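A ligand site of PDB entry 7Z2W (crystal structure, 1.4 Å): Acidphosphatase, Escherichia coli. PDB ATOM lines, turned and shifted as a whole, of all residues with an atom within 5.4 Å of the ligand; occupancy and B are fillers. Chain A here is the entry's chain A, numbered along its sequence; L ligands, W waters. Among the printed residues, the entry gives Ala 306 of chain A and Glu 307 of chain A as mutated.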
ATOM      1  N   ARG A  18      20.142  16.719  -0.795  1.00  0.00           N
ATOM      2  CA  ARG A  18      20.589  16.784  -2.181  1.00  0.00           C
ATOM      3  C   ARG A  18      19.634  15.993  -3.056  1.00  0.00           C
ATOM      4  O   ARG A  18      19.031  15.003  -2.627  1.00  0.00           O
ATOM      5  CB  ARG A  18      21.997  16.215  -2.327  1.00  0.00           C
ATOM      6  CG  ARG A  18      22.537  16.366  -3.745  1.00  0.00           C
ATOM      7  CD  ARG A  18      23.976  15.930  -3.836  1.00  0.00           C
ATOM      8  NE  ARG A  18      24.486  16.118  -5.192  1.00  0.00           N
ATOM      9  CZ  ARG A  18      25.440  15.392  -5.752  1.00  0.00           C
ATOM     10  NH1 ARG A  18      26.051  14.422  -5.086  1.00  0.00           N
ATOM     11  NH2 ARG A  18      25.759  15.620  -7.021  1.00  0.00           N
ATOM     12  N   HIS A  19      19.488  16.440  -4.308  1.00  0.00           N
ATOM     13  CA  HIS A  19      18.741  15.679  -5.304  1.00  0.00           C
ATOM     14  C   HIS A  19      19.315  14.266  -5.448  1.00  0.00           C
ATOM     15  O   HIS A  19      20.437  13.971  -4.992  1.00  0.00           O
ATOM     16  CB  HIS A  19      18.827  16.388  -6.653  1.00  0.00           C
ATOM     17  CG  HIS A  19      20.242  16.530  -7.134  1.00  0.00           C
ATOM     18  ND1 HIS A  19      20.943  15.487  -7.676  1.00  0.00           N
ATOM     19  CD2 HIS A  19      21.106  17.580  -7.071  1.00  0.00           C
ATOM     20  CE1 HIS A  19      22.179  15.878  -7.935  1.00  0.00           C
ATOM     21  NE2 HIS A  19      22.307  17.142  -7.568  1.00  0.00           N
ATOM     22  N   ARG A  22      21.763  11.678 -10.797  1.00  0.00           N
ATOM     23  CA  ARG A  22      21.554  12.447 -12.021  1.00  0.00           C
ATOM     24  C   ARG A  22      22.618  12.093 -13.055  1.00  0.00           C
ATOM     25  O   ARG A  22      23.687  11.558 -12.748  1.00  0.00           O
ATOM     26  CB  ARG A  22      21.682  13.954 -11.739  1.00  0.00           C
ATOM     27  CG  ARG A  22      23.046  14.356 -11.170  1.00  0.00           C
ATOM     28  CD  ARG A  22      23.295  15.829 -11.402  1.00  0.00           C
ATOM     29  NE  ARG A  22      24.501  16.307 -10.729  1.00  0.00           N
ATOM     30  CZ  ARG A  22      25.730  16.080 -11.172  1.00  0.00           C
ATOM     31  NH1 ARG A  22      25.958  15.435 -12.300  1.00  0.00           N
ATOM     32  NH2 ARG A  22      26.767  16.527 -10.457  1.00  0.00           N
ATOM     33  N   THR A  25      26.402  16.849 -15.542  1.00  0.00           N
ATOM     34  CA  THR A  25      25.862  18.146 -15.958  1.00  0.00           C
ATOM     35  C   THR A  25      26.529  18.681 -17.222  1.00  0.00           C
ATOM     36  O   THR A  25      25.969  19.566 -17.874  1.00  0.00           O
ATOM     37  CB  THR A  25      26.042  19.183 -14.852  1.00  0.00           C
ATOM     38  OG1 THR A  25      27.425  19.259 -14.511  1.00  0.00           O
ATOM     39  CG2 THR A  25      25.241  18.792 -13.614  1.00  0.00           C
ATOM     40  N   LYS A  26      27.714  18.172 -17.567  1.00  0.00           N
ATOM     41  CA  LYS A  26      28.486  18.657 -18.716  1.00  0.00           C
ATOM     42  C   LYS A  26      29.133  17.492 -19.446  1.00  0.00           C
ATOM     43  O   LYS A  26      29.405  16.432 -18.876  1.00  0.00           O
ATOM     44  CB  LYS A  26      29.602  19.624 -18.296  1.00  0.00           C
ATOM     45  CG  LYS A  26      29.182  20.879 -17.551  1.00  0.00           C
ATOM     46  CD  LYS A  26      30.199  21.236 -16.462  1.00  0.00           C
ATOM     47  CE  LYS A  26      29.588  22.191 -15.441  1.00  0.00           C
ATOM     48  NZ  LYS A  26      28.772  21.516 -14.380  1.00  0.00           N
ATOM     49  N   ASP A  90      14.284  23.441  -5.331  1.00  0.00           N
ATOM     50  CA  ASP A  90      14.904  24.347  -6.285  1.00  0.00           C
ATOM     51  C   ASP A  90      14.277  24.114  -7.660  1.00  0.00           C
ATOM     52  O   ASP A  90      13.608  23.100  -7.910  1.00  0.00           O
ATOM     53  CB  ASP A  90      16.421  24.125  -6.315  1.00  0.00           C
ATOM     54  CG  ASP A  90      17.202  25.294  -6.925  1.00  0.00           C
ATOM     55  OD1 ASP A  90      16.620  26.357  -7.260  1.00  0.00           O
ATOM     56  OD2 ASP A  90      18.439  25.165  -7.039  1.00  0.00           O
ATOM     57  N   ASP A  92      15.462  23.496 -10.598  1.00  0.00           N
ATOM     58  CA  ASP A  92      16.024  22.551 -11.550  1.00  0.00           C
ATOM     59  C   ASP A  92      15.154  21.311 -11.661  1.00  0.00           C
ATOM     60  O   ASP A  92      14.479  20.912 -10.713  1.00  0.00           O
ATOM     61  CB  ASP A  92      17.417  22.128 -11.087  1.00  0.00           C
ATOM     62  CG  ASP A  92      18.392  23.276 -11.023  1.00  0.00           C
ATOM     63  OD1 ASP A  92      18.162  24.295 -11.707  1.00  0.00           O
ATOM     64  OD2 ASP A  92      19.357  23.166 -10.252  1.00  0.00           O
ATOM     65  N   ARG A  94      16.148  18.278 -11.650  1.00  0.00           N
ATOM     66  CA  ARG A  94      16.582  17.222 -10.753  1.00  0.00           C
ATOM     67  C   ARG A  94      16.090  17.433  -9.333  1.00  0.00           C
ATOM     68  O   ARG A  94      15.803  16.470  -8.619  1.00  0.00           O
ATOM     69  CB  ARG A  94      18.101  17.023 -10.803  1.00  0.00           C
ATOM     70  CG  ARG A  94      18.975  18.222 -10.371  1.00  0.00           C
ATOM     71  CD  ARG A  94      20.438  17.849 -10.556  1.00  0.00           C
ATOM     72  NE  ARG A  94      21.351  18.945 -10.298  1.00  0.00           N
ATOM     73  CZ  ARG A  94      21.766  19.792 -11.241  1.00  0.00           C
ATOM     74  NH1 ARG A  94      21.313  19.709 -12.476  1.00  0.00           N
ATOM     75  NH2 ARG A  94      22.637  20.750 -10.913  1.00  0.00           N
ATOM     76  N   LYS A 131      23.880  33.839  -6.598  1.00  0.00           N
ATOM     77  CA  LYS A 131      23.543  33.606  -7.996  1.00  0.00           C
ATOM     78  C   LYS A 131      22.605  34.649  -8.574  1.00  0.00           C
ATOM     79  O   LYS A 131      22.611  34.858  -9.800  1.00  0.00           O
ATOM     80  CB  LYS A 131      22.995  32.187  -8.181  1.00  0.00           C
ATOM     81  CG  LYS A 131      22.541  31.867  -9.582  1.00  0.00           C
ATOM     82  CD  LYS A 131      23.749  31.782 -10.502  1.00  0.00           C
ATOM     83  CE  LYS A 131      23.651  30.584 -11.430  1.00  0.00           C
ATOM     84  NZ  LYS A 131      23.994  29.324 -10.697  1.00  0.00           N
ATOM     85  N   SER A 214      39.488  20.967 -10.388  1.00  0.00           N
ATOM     86  CA  SER A 214      38.059  20.926 -10.681  1.00  0.00           C
ATOM     87  C   SER A 214      37.709  19.785 -11.637  1.00  0.00           C
ATOM     88  O   SER A 214      36.636  19.191 -11.511  1.00  0.00           O
ATOM     89  CB  SER A 214      37.574  22.259 -11.233  1.00  0.00           C
ATOM     90  OG  SER A 214      38.375  22.611 -12.339  1.00  0.00           O
ATOM     91  N   SER A 217      37.488  16.706  -9.388  1.00  0.00           N
ATOM     92  CA  SER A 217      36.265  16.735  -8.595  1.00  0.00           C
ATOM     93  C   SER A 217      35.059  16.311  -9.417  1.00  0.00           C
ATOM     94  O   SER A 217      34.212  15.549  -8.938  1.00  0.00           O
ATOM     95  CB  SER A 217      36.044  18.140  -8.032  1.00  0.00           C
ATOM     96  OG  SER A 217      34.905  18.119  -7.207  1.00  0.00           O
ATOM     97  N   MET A 218      34.991  16.760 -10.676  1.00  0.00           N
ATOM     98  CA  MET A 218      33.836  16.396 -11.488  1.00  0.00           C
ATOM     99  C   MET A 218      33.913  14.945 -11.958  1.00  0.00           C
ATOM    100  O   MET A 218      32.904  14.228 -11.918  1.00  0.00           O
ATOM    101  CB  MET A 218      33.625  17.404 -12.617  1.00  0.00           C
ATOM    102  CG  MET A 218      32.783  16.911 -13.763  1.00  0.00           C
ATOM    103  SD  MET A 218      32.637  18.148 -15.090  1.00  0.00           S
ATOM    104  CE  MET A 218      34.024  17.707 -16.147  1.00  0.00           C
ATOM    105  N   GLU A 221      33.112  12.355  -9.204  1.00  0.00           N
ATOM    106  CA  GLU A 221      31.667  12.308  -8.966  1.00  0.00           C
ATOM    107  C   GLU A 221      30.940  11.534 -10.075  1.00  0.00           C
ATOM    108  O   GLU A 221      30.001  10.782  -9.787  1.00  0.00           O
ATOM    109  CB  GLU A 221      31.122  13.738  -8.821  1.00  0.00           C
ATOM    110  CG  GLU A 221      29.603  13.829  -8.686  1.00  0.00           C
ATOM    111  CD  GLU A 221      29.070  13.413  -7.321  1.00  0.00           C
ATOM    112  OE1 GLU A 221      29.872  13.032  -6.440  1.00  0.00           O
ATOM    113  OE2 GLU A 221      27.842  13.495  -7.135  1.00  0.00           O
ATOM    114  N   HIS A 252      37.114  14.974  -4.875  1.00  0.00           N
ATOM    115  CA  HIS A 252      35.838  15.682  -4.895  1.00  0.00           C
ATOM    116  C   HIS A 252      35.570  16.328  -3.544  1.00  0.00           C
ATOM    117  O   HIS A 252      35.255  17.531  -3.454  1.00  0.00           O
ATOM    118  CB  HIS A 252      34.745  14.671  -5.205  1.00  0.00           C
ATOM    119  CG  HIS A 252      33.370  15.260  -5.262  1.00  0.00           C
ATOM    120  ND1 HIS A 252      32.878  15.886  -6.380  1.00  0.00           N
ATOM    121  CD2 HIS A 252      32.372  15.297  -4.341  1.00  0.00           C
ATOM    122  CE1 HIS A 252      31.631  16.280  -6.164  1.00  0.00           C
ATOM    123  NE2 HIS A 252      31.307  15.942  -4.937  1.00  0.00           N
ATOM    124  N   PHE A 256      35.194  20.471  -2.317  1.00  0.00           N
ATOM    125  CA  PHE A 256      34.082  20.992  -1.529  1.00  0.00           C
ATOM    126  C   PHE A 256      34.573  21.597  -0.224  1.00  0.00           C
ATOM    127  O   PHE A 256      34.062  22.639   0.217  1.00  0.00           O
ATOM    128  CB  PHE A 256      33.016  19.920  -1.287  1.00  0.00           C
ATOM    129  CG  PHE A 256      31.963  19.883  -2.338  1.00  0.00           C
ATOM    130  CD1 PHE A 256      32.255  19.415  -3.610  1.00  0.00           C
ATOM    131  CD2 PHE A 256      30.698  20.391  -2.081  1.00  0.00           C
ATOM    132  CE1 PHE A 256      31.273  19.397  -4.587  1.00  0.00           C
ATOM    133  CE2 PHE A 256      29.725  20.394  -3.058  1.00  0.00           C
ATOM    134  CZ  PHE A 256      30.004  19.897  -4.301  1.00  0.00           C
ATOM    135  N   GLY A 304      17.572  20.280  -2.690  1.00  0.00           N
ATOM    136  CA  GLY A 304      18.627  21.144  -3.185  1.00  0.00           C
ATOM    137  C   GLY A 304      19.841  20.391  -3.697  1.00  0.00           C
ATOM    138  O   GLY A 304      19.707  19.383  -4.387  1.00  0.00           O
ATOM    139  N   HIS A 305      21.036  20.875  -3.328  1.00  0.00           N
ATOM    140  CA  HIS A 305      22.280  20.512  -4.004  1.00  0.00           C
ATOM    141  C   HIS A 305      23.373  20.174  -3.008  1.00  0.00           C
ATOM    142  O   HIS A 305      23.288  20.473  -1.823  1.00  0.00           O
ATOM    143  CB  HIS A 305      22.738  21.675  -4.879  1.00  0.00           C
ATOM    144  CG  HIS A 305      21.695  22.148  -5.829  1.00  0.00           C
ATOM    145  ND1 HIS A 305      21.556  21.604  -7.094  1.00  0.00           N
ATOM    146  CD2 HIS A 305      20.742  23.093  -5.713  1.00  0.00           C
ATOM    147  CE1 HIS A 305      20.543  22.203  -7.713  1.00  0.00           C
ATOM    148  NE2 HIS A 305      20.040  23.114  -6.900  1.00  0.00           N
ATOM    149  N   ALA A 306      24.446  19.562  -3.530  1.00  0.00           N
ATOM    150  CA  ALA A 306      25.585  19.229  -2.692  1.00  0.00           C
ATOM    151  C   ALA A 306      26.129  20.463  -1.990  1.00  0.00           C
ATOM    152  O   ALA A 306      26.467  20.426  -0.805  1.00  0.00           O
ATOM    153  CB  ALA A 306      26.696  18.544  -3.516  1.00  0.00           C
ATOM    154  N   GLU A 307      26.225  21.589  -2.719  1.00  0.00           N
ATOM    155  CA  GLU A 307      26.737  22.808  -2.113  1.00  0.00           C
ATOM    156  C   GLU A 307      25.918  23.224  -0.900  1.00  0.00           C
ATOM    157  O   GLU A 307      26.484  23.775   0.064  1.00  0.00           O
ATOM    158  CB  GLU A 307      26.791  23.956  -3.125  1.00  0.00           C
ATOM    159  CG  GLU A 307      25.443  24.400  -3.642  1.00  0.00           C
ATOM    160  CD  GLU A 307      25.550  25.579  -4.609  1.00  0.00           C
ATOM    161  OE1 GLU A 307      26.681  26.043  -4.862  1.00  0.00           O
ATOM    162  OE2 GLU A 307      24.501  26.072  -5.089  1.00  0.00           O
HETATM  163  C1  LIG L   1      26.207  22.201  -9.335  1.00  0.00           C
HETATM  164  O1  LIG L   1      24.774  22.557  -9.291  1.00  0.00           O
HETATM  165  S1  LIG L   1      24.369  23.747  -8.318  1.00  0.00           S
HETATM  166  C2  LIG L   1      26.802  22.693 -10.652  1.00  0.00           C
HETATM  167  O2  LIG L   1      24.706  23.277  -6.994  1.00  0.00           O
HETATM  168  S2  LIG L   1      25.375  22.874 -12.908  1.00  0.00           S
HETATM  169  C3  LIG L   1      28.249  22.229 -10.749  1.00  0.00           C
HETATM  170  O3  LIG L   1      22.944  23.931  -8.514  1.00  0.00           O
HETATM  171  S3  LIG L   1      29.581  24.012 -12.057  1.00  0.00           S
HETATM  172  C4  LIG L   1      28.358  20.724 -10.601  1.00  0.00           C
HETATM  173  O4  LIG L   1      25.172  24.857  -8.777  1.00  0.00           O
HETATM  174  S4  LIG L   1      30.372  19.449 -11.723  1.00  0.00           S
HETATM  175  C5  LIG L   1      27.792  20.346  -9.244  1.00  0.00           C
HETATM  176  S5  LIG L   1      28.678  18.459  -7.680  1.00  0.00           S
HETATM  177  C6  LIG L   1      26.315  20.701  -9.223  1.00  0.00           C
HETATM  178  S6  LIG L   1      24.626  19.276  -7.768  1.00  0.00           S
HETATM  179  O5  LIG L   1      26.012  22.018 -11.703  1.00  0.00           O
HETATM  180  O6  LIG L   1      28.794  22.664 -12.044  1.00  0.00           O
HETATM  181  O7  LIG L   1      29.779  20.319 -10.562  1.00  0.00           O
HETATM  182  O8  LIG L   1      27.954  18.901  -8.990  1.00  0.00           O
HETATM  183  O9  LIG L   1      25.781  20.339  -7.889  1.00  0.00           O
HETATM  184  O10 LIG L   1      25.444  24.269 -12.508  1.00  0.00           O
HETATM  185  O11 LIG L   1      30.194  24.123 -13.333  1.00  0.00           O
HETATM  186  O12 LIG L   1      30.571  20.314 -12.830  1.00  0.00           O
HETATM  187  O13 LIG L   1      27.905  18.925  -6.579  1.00  0.00           O
HETATM  188  O14 LIG L   1      25.031  18.178  -8.572  1.00  0.00           O
HETATM  189  O15 LIG L   1      26.203  22.579 -14.051  1.00  0.00           O
HETATM  190  O16 LIG L   1      30.680  23.768 -11.002  1.00  0.00           O
HETATM  191  O17 LIG L   1      31.467  18.752 -11.172  1.00  0.00           O
HETATM  192  O18 LIG L   1      28.582  16.934  -7.771  1.00  0.00           O
HETATM  193  O19 LIG L   1      24.441  19.038  -6.379  1.00  0.00           O
HETATM  194  O20 LIG L   1      24.020  22.408 -13.057  1.00  0.00           O
HETATM  195  O21 LIG L   1      28.750  25.046 -11.574  1.00  0.00           O
HETATM  196  O22 LIG L   1      29.283  18.427 -12.102  1.00  0.00           O
HETATM  197  O23 LIG L   1      30.021  18.887  -7.761  1.00  0.00           O
HETATM  198  O24 LIG L   1      23.369  19.933  -8.338  1.00  0.00           O
HETATM  199  O   HOH W   1      24.903  26.652 -10.731  1.00  0.00           O
HETATM  200  O   HOH W   2      26.555  21.725  -5.561  1.00  0.00           O
HETATM  201  O   HOH W   3      21.314  25.130  -9.893  1.00  0.00           O
HETATM  202  O   HOH W   4      31.293  21.583  -7.554  1.00  0.00           O
HETATM  203  O   HOH W   5      24.068  27.606  -7.126  1.00  0.00           O
HETATM  204  O   HOH W   6      30.033  15.829 -11.462  1.00  0.00           O
HETATM  205  O   HOH W   7      32.723  18.837  -8.751  1.00  0.00           O
HETATM  206  O   HOH W   8      33.189  21.893 -12.071  1.00  0.00           O
HETATM  207  O   HOH W   9      28.711  15.927 -13.507  1.00  0.00           O
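A ring nitrogen (NE2) of His 19 lies within hydrogen-bond range of an oxygen (O14) of the ligand (3.1 Å).
The side-chain hydroxyl of Thr 25 is in hydrogen-bond range of an oxygen (O22) of the ligand, at 3.2 Å.
O19 of the ligand sits at hydrogen-bond distance from N of Ala 306.
The side-chain amino group (NZ) of Lys 26 is in salt-bridge range of an oxygen (O12) of the ligand (2.7 Å).
The guanidinium group of Arg 94 lies within salt-bridge range of an oxygen (O24) of the ligand (2.8 Å).
ND1 of His 305 lies within hydrogen-bond range of O24 of the ligand (2.8 Å).
The guanidinium group of Arg 18 lies within salt-bridge range of an oxygen (O14) of the ligand.
The guanidinium group of Arg 22 is in salt-bridge range of an oxygen (O14) of the ligand (2.9 Å).
NH1 of Arg 18 is in salt-bridge range of OE2 of Glu 221 (2.9 Å).
NE2 of His 19 is in hydrogen-bond range of NE of Arg 94.
A ring nitrogen (NE2) of His 305 lies within hydrogen-bond range of the side-chain carboxylate (OD2) of Asp 90.
A ring nitrogen (ND1) of His 252 is in hydrogen-bond range of the backbone carbonyl oxygen (O) of Ser 217, at 2.9 Å.
The backbone NH (N) of His 19 lies within hydrogen-bond range of the backbone carbonyl oxygen (O) of Gly 304, 3.0 Å away.
A ring nitrogen (NE2) of His 19 sits at hydrogen-bond distance from the guanidinium group (NE) of Arg 18 (3.4 Å).
NE2 of His 305 lies close to OD2 of Asp 92 (3.4 Å).
NZ of Lys 26 lies within hydrogen-bond range of OG1 of Thr 25, 2.6 Å away.
SD of Met 218 lies close to O12 of the ligand.
An oxygen (O2) of the ligand lies close to the side-chain carboxylate (OE2) of Glu 307 (3.4 Å).
Residues that only touch the ligand: Phe 256, Glu 221 and His 252.
Of the 19 residues printed, 13 come within 4 Å of the ligand.
The nearest printed residue that does not touch the ligand is Asp 92 (4.1 Å).
Water W3 lies within hydrogen-bond range of an oxygen (O3) of the ligand (2.4 Å) and the side-chain carboxylate of Asp 92 (2.8 Å).
Water W1 bridges O4 of the ligand (2.7 Å) and NZ of Lys 131 (2.8 Å).
Water W7 bridges O17 of the ligand (2.7 Å) and OG of Ser 217 (2.8 Å).
Water W6 lies within hydrogen-bond range of O22 of the ligand, O of Met 218 and NH2 of Arg 22.
Water W2 lies within hydrogen-bond range of O2 of the ligand and N of Glu 307.
Water W9 lies within hydrogen-bond range of an oxygen (O22) of the ligand (2.9 Å), the guanidinium group (NH1) of Arg 22 (3.0 Å) and the backbone NH (N) of Thr 25 (3.2 Å).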
